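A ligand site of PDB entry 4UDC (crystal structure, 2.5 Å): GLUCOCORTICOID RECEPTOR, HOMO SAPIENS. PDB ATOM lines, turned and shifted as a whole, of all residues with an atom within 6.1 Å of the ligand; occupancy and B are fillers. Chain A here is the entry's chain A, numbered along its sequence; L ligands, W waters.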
ATOM      1  N   MET A  63      -1.588 -28.578  -1.635  1.00  0.00           N
ATOM      2  CA  MET A  63      -1.134 -28.764  -0.254  1.00  0.00           C
ATOM      3  C   MET A  63       0.098 -29.674  -0.193  1.00  0.00           C
ATOM      4  O   MET A  63       1.072 -29.347   0.502  1.00  0.00           O
ATOM      5  CB  MET A  63      -2.261 -29.357   0.606  1.00  0.00           C
ATOM      6  CG  MET A  63      -3.337 -28.355   0.981  1.00  0.00           C
ATOM      7  SD  MET A  63      -4.768 -29.151   1.771  1.00  0.00           S
ATOM      8  CE  MET A  63      -4.223 -29.313   3.420  1.00  0.00           C
ATOM      9  N   THR A  64       0.058 -30.773  -0.975  1.00  0.00           N
ATOM     10  CA  THR A  64       1.109 -31.780  -1.142  1.00  0.00           C
ATOM     11  C   THR A  64       2.408 -31.179  -1.732  1.00  0.00           C
ATOM     12  O   THR A  64       3.473 -31.424  -1.192  1.00  0.00           O
ATOM     13  CB  THR A  64       0.544 -32.967  -1.954  1.00  0.00           C
ATOM     14  OG1 THR A  64      -0.410 -33.605  -1.122  1.00  0.00           O
ATOM     15  CG2 THR A  64       1.596 -33.973  -2.343  1.00  0.00           C
ATOM     16  N   LEU A  66       3.151 -27.924  -1.863  1.00  0.00           N
ATOM     17  CA  LEU A  66       3.605 -26.901  -0.931  1.00  0.00           C
ATOM     18  C   LEU A  66       4.424 -27.445   0.232  1.00  0.00           C
ATOM     19  O   LEU A  66       5.345 -26.785   0.688  1.00  0.00           O
ATOM     20  CB  LEU A  66       2.437 -26.028  -0.420  1.00  0.00           C
ATOM     21  CG  LEU A  66       1.745 -25.107  -1.437  1.00  0.00           C
ATOM     22  CD1 LEU A  66       0.688 -24.267  -0.758  1.00  0.00           C
ATOM     23  CD2 LEU A  66       2.748 -24.228  -2.183  1.00  0.00           C
ATOM     24  N   ASN A  67       4.093 -28.658   0.718  1.00  0.00           N
ATOM     25  CA  ASN A  67       4.811 -29.288   1.804  1.00  0.00           C
ATOM     26  C   ASN A  67       6.201 -29.680   1.350  1.00  0.00           C
ATOM     27  O   ASN A  67       7.165 -29.390   2.060  1.00  0.00           O
ATOM     28  CB  ASN A  67       4.029 -30.484   2.368  1.00  0.00           C
ATOM     29  CG  ASN A  67       2.860 -30.049   3.221  1.00  0.00           C
ATOM     30  OD1 ASN A  67       2.827 -28.949   3.771  1.00  0.00           O
ATOM     31  ND2 ASN A  67       1.870 -30.914   3.362  1.00  0.00           N
ATOM     32  N   MET A  68       6.332 -30.215   0.111  1.00  0.00           N
ATOM     33  CA  MET A  68       7.631 -30.577  -0.488  1.00  0.00           C
ATOM     34  C   MET A  68       8.495 -29.328  -0.711  1.00  0.00           C
ATOM     35  O   MET A  68       9.690 -29.339  -0.379  1.00  0.00           O
ATOM     36  CB  MET A  68       7.438 -31.394  -1.781  1.00  0.00           C
ATOM     37  CG  MET A  68       6.656 -32.698  -1.593  1.00  0.00           C
ATOM     38  SD  MET A  68       7.182 -33.862  -0.295  1.00  0.00           S
ATOM     39  CE  MET A  68       8.774 -34.319  -0.890  1.00  0.00           C
ATOM     40  N   LEU A  69       7.883 -28.238  -1.182  1.00  0.00           N
ATOM     41  CA  LEU A  69       8.527 -26.926  -1.338  1.00  0.00           C
ATOM     42  C   LEU A  69       8.955 -26.379   0.028  1.00  0.00           C
ATOM     43  O   LEU A  69      10.089 -25.908   0.154  1.00  0.00           O
ATOM     44  CB  LEU A  69       7.557 -25.936  -2.038  1.00  0.00           C
ATOM     45  CG  LEU A  69       8.037 -24.491  -2.209  1.00  0.00           C
ATOM     46  CD1 LEU A  69       9.269 -24.388  -3.120  1.00  0.00           C
ATOM     47  CD2 LEU A  69       6.888 -23.609  -2.702  1.00  0.00           C
ATOM     48  N   GLY A  70       8.043 -26.465   1.027  1.00  0.00           N
ATOM     49  CA  GLY A  70       8.239 -26.042   2.410  1.00  0.00           C
ATOM     50  C   GLY A  70       9.482 -26.627   3.059  1.00  0.00           C
ATOM     51  O   GLY A  70      10.258 -25.901   3.699  1.00  0.00           O
ATOM     52  N   GLY A  71       9.692 -27.934   2.863  1.00  0.00           N
ATOM     53  CA  GLY A  71      10.881 -28.633   3.368  1.00  0.00           C
ATOM     54  C   GLY A  71      12.166 -28.122   2.753  1.00  0.00           C
ATOM     55  O   GLY A  71      13.153 -27.927   3.475  1.00  0.00           O
ATOM     56  N   GLN A  73      12.579 -25.115   1.433  1.00  0.00           N
ATOM     57  CA  GLN A  73      12.651 -23.731   1.884  1.00  0.00           C
ATOM     58  C   GLN A  73      13.149 -23.677   3.330  1.00  0.00           C
ATOM     59  O   GLN A  73      13.915 -22.768   3.658  1.00  0.00           O
ATOM     60  CB  GLN A  73      11.272 -23.095   1.782  1.00  0.00           C
ATOM     61  CG  GLN A  73      10.945 -22.486   0.424  1.00  0.00           C
ATOM     62  CD  GLN A  73       9.550 -21.939   0.379  1.00  0.00           C
ATOM     63  OE1 GLN A  73       8.994 -21.681  -0.685  1.00  0.00           O
ATOM     64  NE2 GLN A  73       8.913 -21.774   1.536  1.00  0.00           N
ATOM     65  N   VAL A  74      12.771 -24.665   4.186  1.00  0.00           N
ATOM     66  CA  VAL A  74      13.224 -24.755   5.590  1.00  0.00           C
ATOM     67  C   VAL A  74      14.697 -25.165   5.648  1.00  0.00           C
ATOM     68  O   VAL A  74      15.442 -24.580   6.449  1.00  0.00           O
ATOM     69  CB  VAL A  74      12.299 -25.594   6.499  1.00  0.00           C
ATOM     70  CG1 VAL A  74      12.980 -25.936   7.811  1.00  0.00           C
ATOM     71  CG2 VAL A  74      10.996 -24.863   6.767  1.00  0.00           C
ATOM     72  N   TRP A 103      10.143 -21.643  12.186  1.00  0.00           N
ATOM     73  CA  TRP A 103      10.101 -22.019  10.771  1.00  0.00           C
ATOM     74  C   TRP A 103       8.833 -21.570  10.039  1.00  0.00           C
ATOM     75  O   TRP A 103       8.934 -21.042   8.916  1.00  0.00           O
ATOM     76  CB  TRP A 103      10.356 -23.527  10.575  1.00  0.00           C
ATOM     77  CG  TRP A 103       9.188 -24.412  10.897  1.00  0.00           C
ATOM     78  CD1 TRP A 103       8.868 -24.929  12.115  1.00  0.00           C
ATOM     79  CD2 TRP A 103       8.194 -24.884   9.985  1.00  0.00           C
ATOM     80  NE1 TRP A 103       7.748 -25.717  12.019  1.00  0.00           N
ATOM     81  CE2 TRP A 103       7.320 -25.725  10.719  1.00  0.00           C
ATOM     82  CE3 TRP A 103       7.945 -24.683   8.607  1.00  0.00           C
ATOM     83  CZ2 TRP A 103       6.223 -26.363  10.133  1.00  0.00           C
ATOM     84  CZ3 TRP A 103       6.837 -25.297   8.034  1.00  0.00           C
ATOM     85  CH2 TRP A 103       5.997 -26.124   8.792  1.00  0.00           C
ATOM     86  N   MET A 104       7.652 -21.769  10.660  1.00  0.00           N
ATOM     87  CA  MET A 104       6.360 -21.410  10.046  1.00  0.00           C
ATOM     88  C   MET A 104       6.267 -19.907   9.898  1.00  0.00           C
ATOM     89  O   MET A 104       5.781 -19.429   8.868  1.00  0.00           O
ATOM     90  CB  MET A 104       5.173 -21.958  10.869  1.00  0.00           C
ATOM     91  CG  MET A 104       3.809 -21.767  10.194  1.00  0.00           C
ATOM     92  SD  MET A 104       3.715 -22.543   8.555  1.00  0.00           S
ATOM     93  CE  MET A 104       2.980 -24.080   8.998  1.00  0.00           C
ATOM     94  N   MET A 107       8.519 -18.908   7.067  1.00  0.00           N
ATOM     95  CA  MET A 107       7.871 -19.332   5.814  1.00  0.00           C
ATOM     96  C   MET A 107       6.726 -18.409   5.426  1.00  0.00           C
ATOM     97  O   MET A 107       6.666 -17.962   4.279  1.00  0.00           O
ATOM     98  CB  MET A 107       7.439 -20.827   5.827  1.00  0.00           C
ATOM     99  CG  MET A 107       8.592 -21.830   5.927  1.00  0.00           C
ATOM    100  SD  MET A 107       9.936 -21.506   4.753  1.00  0.00           S
ATOM    101  CE  MET A 107      11.206 -20.896   5.806  1.00  0.00           C
ATOM    102  N   ALA A 108       5.846 -18.095   6.391  1.00  0.00           N
ATOM    103  CA  ALA A 108       4.696 -17.216   6.165  1.00  0.00           C
ATOM    104  C   ALA A 108       5.098 -15.762   5.895  1.00  0.00           C
ATOM    105  O   ALA A 108       4.519 -15.110   5.030  1.00  0.00           O
ATOM    106  CB  ALA A 108       3.743 -17.295   7.337  1.00  0.00           C
ATOM    107  N   LEU A 111       6.676 -15.558   2.387  1.00  0.00           N
ATOM    108  CA  LEU A 111       5.595 -15.747   1.408  1.00  0.00           C
ATOM    109  C   LEU A 111       4.799 -14.446   1.249  1.00  0.00           C
ATOM    110  O   LEU A 111       4.397 -14.129   0.134  1.00  0.00           O
ATOM    111  CB  LEU A 111       4.697 -16.923   1.801  1.00  0.00           C
ATOM    112  CG  LEU A 111       3.285 -16.998   1.215  1.00  0.00           C
ATOM    113  CD1 LEU A 111       3.326 -17.418  -0.254  1.00  0.00           C
ATOM    114  CD2 LEU A 111       2.425 -17.911   2.021  1.00  0.00           C
ATOM    115  N   ARG A 114       7.045 -11.995  -0.919  1.00  0.00           N
ATOM    116  CA  ARG A 114       7.002 -12.371  -2.334  1.00  0.00           C
ATOM    117  C   ARG A 114       5.675 -11.991  -2.946  1.00  0.00           C
ATOM    118  O   ARG A 114       5.640 -11.545  -4.093  1.00  0.00           O
ATOM    119  CB  ARG A 114       7.212 -13.884  -2.534  1.00  0.00           C
ATOM    120  CG  ARG A 114       8.595 -14.387  -2.165  1.00  0.00           C
ATOM    121  CD  ARG A 114       8.885 -15.789  -2.676  1.00  0.00           C
ATOM    122  NE  ARG A 114       7.970 -16.842  -2.208  1.00  0.00           N
ATOM    123  CZ  ARG A 114       8.068 -17.468  -1.039  1.00  0.00           C
ATOM    124  NH1 ARG A 114       9.005 -17.121  -0.169  1.00  0.00           N
ATOM    125  NH2 ARG A 114       7.218 -18.433  -0.721  1.00  0.00           N
ATOM    126  N   CYS A 125       2.140 -15.806  -3.823  1.00  0.00           N
ATOM    127  CA  CYS A 125       3.263 -16.191  -4.648  1.00  0.00           C
ATOM    128  C   CYS A 125       4.111 -17.176  -3.855  1.00  0.00           C
ATOM    129  O   CYS A 125       5.076 -16.791  -3.204  1.00  0.00           O
ATOM    130  CB  CYS A 125       4.056 -14.970  -5.116  1.00  0.00           C
ATOM    131  SG  CYS A 125       5.469 -15.373  -6.188  1.00  0.00           S
ATOM    132  N   PHE A 126       3.692 -18.458  -3.863  1.00  0.00           N
ATOM    133  CA  PHE A 126       4.385 -19.549  -3.174  1.00  0.00           C
ATOM    134  C   PHE A 126       5.736 -19.788  -3.845  1.00  0.00           C
ATOM    135  O   PHE A 126       6.759 -19.864  -3.179  1.00  0.00           O
ATOM    136  CB  PHE A 126       3.518 -20.811  -3.128  1.00  0.00           C
ATOM    137  CG  PHE A 126       2.383 -20.736  -2.130  1.00  0.00           C
ATOM    138  CD1 PHE A 126       2.610 -20.882  -0.756  1.00  0.00           C
ATOM    139  CD2 PHE A 126       1.064 -20.593  -2.553  1.00  0.00           C
ATOM    140  CE1 PHE A 126       1.568 -20.819   0.160  1.00  0.00           C
ATOM    141  CE2 PHE A 126       0.004 -20.557  -1.626  1.00  0.00           C
ATOM    142  CZ  PHE A 126       0.262 -20.663  -0.276  1.00  0.00           C
ATOM    143  N   ALA A 127       5.722 -19.779  -5.159  1.00  0.00           N
ATOM    144  CA  ALA A 127       6.894 -19.955  -6.013  1.00  0.00           C
ATOM    145  C   ALA A 127       6.537 -19.301  -7.388  1.00  0.00           C
ATOM    146  O   ALA A 127       5.357 -19.057  -7.643  1.00  0.00           O
ATOM    147  CB  ALA A 127       7.188 -21.436  -6.183  1.00  0.00           C
ATOM    148  N   GLN A 145      -7.475 -21.669   4.328  1.00  0.00           N
ATOM    149  CA  GLN A 145      -6.084 -21.771   4.755  1.00  0.00           C
ATOM    150  C   GLN A 145      -5.257 -20.591   4.234  1.00  0.00           C
ATOM    151  O   GLN A 145      -4.489 -20.023   4.996  1.00  0.00           O
ATOM    152  CB  GLN A 145      -5.446 -23.156   4.483  1.00  0.00           C
ATOM    153  CG  GLN A 145      -5.655 -23.737   3.107  1.00  0.00           C
ATOM    154  CD  GLN A 145      -5.338 -25.210   3.092  1.00  0.00           C
ATOM    155  OE1 GLN A 145      -4.191 -25.635   3.273  1.00  0.00           O
ATOM    156  NE2 GLN A 145      -6.327 -26.026   2.797  1.00  0.00           N
ATOM    157  N   CYS A 146      -5.535 -20.154   3.001  1.00  0.00           N
ATOM    158  CA  CYS A 146      -4.898 -19.042   2.278  1.00  0.00           C
ATOM    159  C   CYS A 146      -5.118 -17.654   2.890  1.00  0.00           C
ATOM    160  O   CYS A 146      -4.245 -16.808   2.715  1.00  0.00           O
ATOM    161  CB  CYS A 146      -5.316 -19.055   0.820  1.00  0.00           C
ATOM    162  SG  CYS A 146      -4.549 -20.366  -0.160  1.00  0.00           S
ATOM    163  N   MET A 149      -2.495 -16.427   5.377  1.00  0.00           N
ATOM    164  CA  MET A 149      -1.294 -16.129   4.597  1.00  0.00           C
ATOM    165  C   MET A 149      -1.496 -14.795   3.835  1.00  0.00           C
ATOM    166  O   MET A 149      -0.555 -14.006   3.748  1.00  0.00           O
ATOM    167  CB  MET A 149      -0.980 -17.299   3.648  1.00  0.00           C
ATOM    168  CG  MET A 149      -0.592 -18.582   4.375  1.00  0.00           C
ATOM    169  SD  MET A 149      -0.310 -19.977   3.256  1.00  0.00           S
ATOM    170  CE  MET A 149      -1.741 -20.815   3.357  1.00  0.00           C
ATOM    171  N   ASN A 234      -2.742 -20.263  13.519  1.00  0.00           N
ATOM    172  CA  ASN A 234      -3.721 -20.745  12.550  1.00  0.00           C
ATOM    173  C   ASN A 234      -3.141 -21.682  11.501  1.00  0.00           C
ATOM    174  O   ASN A 234      -3.778 -22.682  11.150  1.00  0.00           O
ATOM    175  CB  ASN A 234      -4.463 -19.585  11.920  1.00  0.00           C
ATOM    176  CG  ASN A 234      -5.365 -18.892  12.915  1.00  0.00           C
ATOM    177  OD1 ASN A 234      -6.220 -19.524  13.553  1.00  0.00           O
ATOM    178  ND2 ASN A 234      -5.122 -17.615  13.144  1.00  0.00           N
ATOM    179  N   LEU A 235      -1.899 -21.391  11.048  1.00  0.00           N
ATOM    180  CA  LEU A 235      -1.167 -22.181  10.051  1.00  0.00           C
ATOM    181  C   LEU A 235      -0.751 -23.521  10.618  1.00  0.00           C
ATOM    182  O   LEU A 235      -0.931 -24.533   9.944  1.00  0.00           O
ATOM    183  CB  LEU A 235       0.029 -21.397   9.471  1.00  0.00           C
ATOM    184  CG  LEU A 235      -0.340 -20.127   8.695  1.00  0.00           C
ATOM    185  CD1 LEU A 235       0.873 -19.468   8.132  1.00  0.00           C
ATOM    186  CD2 LEU A 235      -1.391 -20.404   7.589  1.00  0.00           C
ATOM    187  N   LEU A 236      -0.264 -23.535  11.871  1.00  0.00           N
ATOM    188  CA  LEU A 236       0.149 -24.746  12.578  1.00  0.00           C
ATOM    189  C   LEU A 236      -1.028 -25.642  12.935  1.00  0.00           C
ATOM    190  O   LEU A 236      -0.829 -26.855  12.999  1.00  0.00           O
ATOM    191  CB  LEU A 236       1.036 -24.484  13.801  1.00  0.00           C
ATOM    192  CG  LEU A 236       2.459 -23.961  13.556  1.00  0.00           C
ATOM    193  CD1 LEU A 236       3.132 -23.674  14.876  1.00  0.00           C
ATOM    194  CD2 LEU A 236       3.321 -24.955  12.784  1.00  0.00           C
ATOM    195  N   TYR A 238      -3.563 -26.237  10.877  1.00  0.00           N
ATOM    196  CA  TYR A 238      -3.663 -26.928   9.585  1.00  0.00           C
ATOM    197  C   TYR A 238      -2.522 -27.925   9.425  1.00  0.00           C
ATOM    198  O   TYR A 238      -2.746 -29.086   9.113  1.00  0.00           O
ATOM    199  CB  TYR A 238      -3.619 -25.907   8.433  1.00  0.00           C
ATOM    200  CG  TYR A 238      -4.981 -25.397   8.023  1.00  0.00           C
ATOM    201  CD1 TYR A 238      -5.776 -26.116   7.138  1.00  0.00           C
ATOM    202  CD2 TYR A 238      -5.462 -24.175   8.489  1.00  0.00           C
ATOM    203  CE1 TYR A 238      -7.031 -25.659   6.752  1.00  0.00           C
ATOM    204  CE2 TYR A 238      -6.724 -23.702   8.111  1.00  0.00           C
ATOM    205  CZ  TYR A 238      -7.500 -24.447   7.243  1.00  0.00           C
ATOM    206  OH  TYR A 238      -8.739 -24.001   6.845  1.00  0.00           O
ATOM    207  N   CYS A 239      -1.292 -27.460   9.679  1.00  0.00           N
ATOM    208  CA  CYS A 239      -0.066 -28.219   9.599  1.00  0.00           C
ATOM    209  C   CYS A 239      -0.080 -29.495  10.483  1.00  0.00           C
ATOM    210  O   CYS A 239       0.133 -30.601   9.975  1.00  0.00           O
ATOM    211  CB  CYS A 239       1.117 -27.314   9.928  1.00  0.00           C
ATOM    212  SG  CYS A 239       2.724 -28.104   9.740  1.00  0.00           S
ATOM    213  N   PHE A 240      -0.363 -29.327  11.778  1.00  0.00           N
ATOM    214  CA  PHE A 240      -0.421 -30.404  12.754  1.00  0.00           C
ATOM    215  C   PHE A 240      -1.517 -31.430  12.445  1.00  0.00           C
ATOM    216  O   PHE A 240      -1.271 -32.634  12.572  1.00  0.00           O
ATOM    217  CB  PHE A 240      -0.563 -29.829  14.176  1.00  0.00           C
ATOM    218  CG  PHE A 240       0.637 -29.095  14.736  1.00  0.00           C
ATOM    219  CD1 PHE A 240       1.874 -29.115  14.069  1.00  0.00           C
ATOM    220  CD2 PHE A 240       0.563 -28.440  15.958  1.00  0.00           C
ATOM    221  CE1 PHE A 240       2.990 -28.491  14.607  1.00  0.00           C
ATOM    222  CE2 PHE A 240       1.691 -27.814  16.502  1.00  0.00           C
ATOM    223  CZ  PHE A 240       2.899 -27.835  15.814  1.00  0.00           C
ATOM    224  N   THR A 242      -2.984 -32.055   9.367  1.00  0.00           N
ATOM    225  CA  THR A 242      -2.654 -32.749   8.128  1.00  0.00           C
ATOM    226  C   THR A 242      -1.485 -33.698   8.320  1.00  0.00           C
ATOM    227  O   THR A 242      -1.458 -34.747   7.676  1.00  0.00           O
ATOM    228  CB  THR A 242      -2.489 -31.755   6.968  1.00  0.00           C
ATOM    229  OG1 THR A 242      -1.453 -30.835   7.266  1.00  0.00           O
ATOM    230  CG2 THR A 242      -3.773 -30.998   6.679  1.00  0.00           C
ATOM    231  N   PHE A 243      -0.566 -33.394   9.253  1.00  0.00           N
ATOM    232  CA  PHE A 243       0.569 -34.263   9.583  1.00  0.00           C
ATOM    233  C   PHE A 243       0.100 -35.533  10.322  1.00  0.00           C
ATOM    234  O   PHE A 243       0.399 -36.658   9.871  1.00  0.00           O
ATOM    235  CB  PHE A 243       1.635 -33.521  10.418  1.00  0.00           C
ATOM    236  CG  PHE A 243       2.810 -34.414  10.710  1.00  0.00           C
ATOM    237  CD1 PHE A 243       3.644 -34.861   9.684  1.00  0.00           C
ATOM    238  CD2 PHE A 243       3.041 -34.890  11.998  1.00  0.00           C
ATOM    239  CE1 PHE A 243       4.661 -35.764   9.940  1.00  0.00           C
ATOM    240  CE2 PHE A 243       4.085 -35.758  12.255  1.00  0.00           C
ATOM    241  CZ  PHE A 243       4.896 -36.187  11.222  1.00  0.00           C
ATOM    242  N   ILE A 250      -1.633 -36.801   3.272  1.00  0.00           N
ATOM    243  CA  ILE A 250      -0.889 -35.569   3.052  1.00  0.00           C
ATOM    244  C   ILE A 250       0.549 -35.790   3.531  1.00  0.00           C
ATOM    245  O   ILE A 250       0.803 -35.870   4.742  1.00  0.00           O
ATOM    246  CB  ILE A 250      -1.591 -34.302   3.638  1.00  0.00           C
ATOM    247  CG1 ILE A 250      -2.880 -33.992   2.831  1.00  0.00           C
ATOM    248  CG2 ILE A 250      -0.644 -33.089   3.607  1.00  0.00           C
ATOM    249  CD1 ILE A 250      -3.840 -33.086   3.489  1.00  0.00           C
ATOM    250  N   PHE A 252       4.561 -35.029   4.122  1.00  0.00           N
ATOM    251  CA  PHE A 252       5.483 -34.014   4.600  1.00  0.00           C
ATOM    252  C   PHE A 252       6.891 -34.584   4.411  1.00  0.00           C
ATOM    253  O   PHE A 252       7.130 -35.735   4.768  1.00  0.00           O
ATOM    254  CB  PHE A 252       5.222 -33.675   6.086  1.00  0.00           C
ATOM    255  CG  PHE A 252       4.026 -32.783   6.304  1.00  0.00           C
ATOM    256  CD1 PHE A 252       2.736 -33.290   6.318  1.00  0.00           C
ATOM    257  CD2 PHE A 252       4.196 -31.407   6.474  1.00  0.00           C
ATOM    258  CE1 PHE A 252       1.639 -32.460   6.503  1.00  0.00           C
ATOM    259  CE2 PHE A 252       3.094 -30.580   6.682  1.00  0.00           C
ATOM    260  CZ  PHE A 252       1.823 -31.118   6.701  1.00  0.00           C
ATOM    261  N   LEU A 256      10.310 -31.309   7.469  1.00  0.00           N
ATOM    262  CA  LEU A 256       9.107 -30.852   8.149  1.00  0.00           C
ATOM    263  C   LEU A 256       8.585 -31.885   9.125  1.00  0.00           C
ATOM    264  O   LEU A 256       8.300 -31.507  10.241  1.00  0.00           O
ATOM    265  CB  LEU A 256       8.026 -30.377   7.188  1.00  0.00           C
ATOM    266  CG  LEU A 256       8.415 -29.241   6.253  1.00  0.00           C
ATOM    267  CD1 LEU A 256       7.250 -28.817   5.406  1.00  0.00           C
ATOM    268  CD2 LEU A 256       9.002 -28.075   7.012  1.00  0.00           C
HETATM  269  C1  LIG L   1       5.389 -23.887   2.090  1.00  0.00           C
HETATM  270  C2  LIG L   1       5.860 -23.040   1.187  1.00  0.00           C
HETATM  271  C3  LIG L   1       5.765 -21.585   1.428  1.00  0.00           C
HETATM  272  C4  LIG L   1       5.109 -21.088   2.656  1.00  0.00           C
HETATM  273  C5  LIG L   1       4.681 -21.962   3.576  1.00  0.00           C
HETATM  274  C6  LIG L   1       3.996 -21.406   4.827  1.00  0.00           C
HETATM  275  C7  LIG L   1       2.595 -22.027   4.981  1.00  0.00           C
HETATM  276  C8  LIG L   1       2.600 -23.567   4.844  1.00  0.00           C
HETATM  277  C9  LIG L   1       3.271 -24.000   3.493  1.00  0.00           C
HETATM  278  C10 LIG L   1       4.760 -23.484   3.399  1.00  0.00           C
HETATM  279  C11 LIG L   1       3.120 -25.517   3.216  1.00  0.00           C
HETATM  280  C12 LIG L   1       1.684 -26.068   3.435  1.00  0.00           C
HETATM  281  C13 LIG L   1       1.082 -25.704   4.810  1.00  0.00           C
HETATM  282  C14 LIG L   1       1.169 -24.126   4.929  1.00  0.00           C
HETATM  283  C15 LIG L   1       0.302 -23.813   6.167  1.00  0.00           C
HETATM  284  C16 LIG L   1      -0.850 -24.861   6.051  1.00  0.00           C
HETATM  285  C17 LIG L   1      -0.465 -25.893   4.955  1.00  0.00           C
HETATM  286  C18 LIG L   1       1.831 -26.462   5.953  1.00  0.00           C
HETATM  287  C19 LIG L   1       5.739 -24.067   4.450  1.00  0.00           C
HETATM  288  C20 LIG L   1      -0.852 -27.342   5.290  1.00  0.00           C
HETATM  289  C21 LIG L   1      -0.873 -28.401   4.212  1.00  0.00           C
HETATM  290  C22 LIG L   1      -2.165 -24.137   5.754  1.00  0.00           C
HETATM  291  F1  LIG L   1       2.573 -23.330   2.481  1.00  0.00           F
HETATM  292  O1  LIG L   1       6.270 -20.809   0.635  1.00  0.00           O
HETATM  293  O2  LIG L   1       4.037 -26.313   3.965  1.00  0.00           O
HETATM  294  O3  LIG L   1      -1.177 -25.551   3.751  1.00  0.00           O
HETATM  295  O4  LIG L   1      -1.171 -27.680   6.409  1.00  0.00           O
HETATM  296  O5  LIG L   1      -0.844 -29.710   4.774  1.00  0.00           O
HETATM  297  O   HOH W   1       8.487 -18.895   2.130  1.00  0.00           O
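The side-chain hydroxyl of Thr 242 sits at hydrogen-bond distance from an oxygen (O5) of the ligand (2.8 Å).
O1 of the ligand sits at hydrogen-bond distance from NE2 of Gln 73, 3.0 Å away.
The guanidinium group of Arg 114 sits at hydrogen-bond distance from an oxygen (O1) of the ligand.
OE1 of Gln 145 sits at hydrogen-bond distance from O3 of the ligand.
The backbone NH (N) of Cys 239 lies within hydrogen-bond range of an oxygen (O4) of the ligand (3.3 Å).
O2 of the ligand is in hydrogen-bond range of OD1 of Asn 67 (2.9 Å).
O of Cys 239 sits at hydrogen-bond distance from OG1 of Thr 242, at 3.1 Å.
The guanidinium group of Arg 114 is in hydrogen-bond range of the backbone carbonyl oxygen of Phe 126.
The side-chain sulfur of Met 63 sits at hydrogen-bond distance from the side-chain amide nitrogen of Gln 145.
The side-chain hydroxyl (OG1) of Thr 242 is in hydrogen-bond range of the backbone carbonyl oxygen (O) of Tyr 238 (2.9 Å).
The backbone carbonyl oxygen (O) of Met 63 sits close to the side-chain amide nitrogen (ND2) of Asn 67 (3.4 Å).
NE2 of Gln 73 sits at hydrogen-bond distance from SD of Met 107 (3.4 Å).
O of Cys 125 sits at hydrogen-bond distance from NE of Arg 114 (3.1 Å).
O of Tyr 238 lies close to O4 of the ligand, at 3.4 Å.
CE of Met 63 touches C21 of the ligand, 3.6 Å away.
Leu 66 touches the ligand (O to C1, 3.2 Å).
Gly 70 touches the ligand (CA to C1, 3.6 Å).
Trp 103 touches the ligand.
Met 104 touches the ligand (SD to C7, 3.8 Å).
Met 107 touches the ligand.
Phe 126 touches the ligand (CE1 to F1, 3.6 Å).
SD of Met 149 touches C7 of the ligand, at 3.95 Å.
Leu 235 touches the ligand.
Ile 250 touches the ligand (CG2 to O5, 3.6 Å).
Phe 252 touches the ligand (CZ to O5, 3.6 Å).
The nearest printed residue that does not touch the ligand is Leu 69 (4.1 Å).
Water W1 lies within hydrogen-bond range of NH1 of Arg 114 (2.9 Å), O of Met 107 (3.0 Å), NE2 of Gln 73 (3.0 Å) and O1 of the ligand (3.3 Å).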
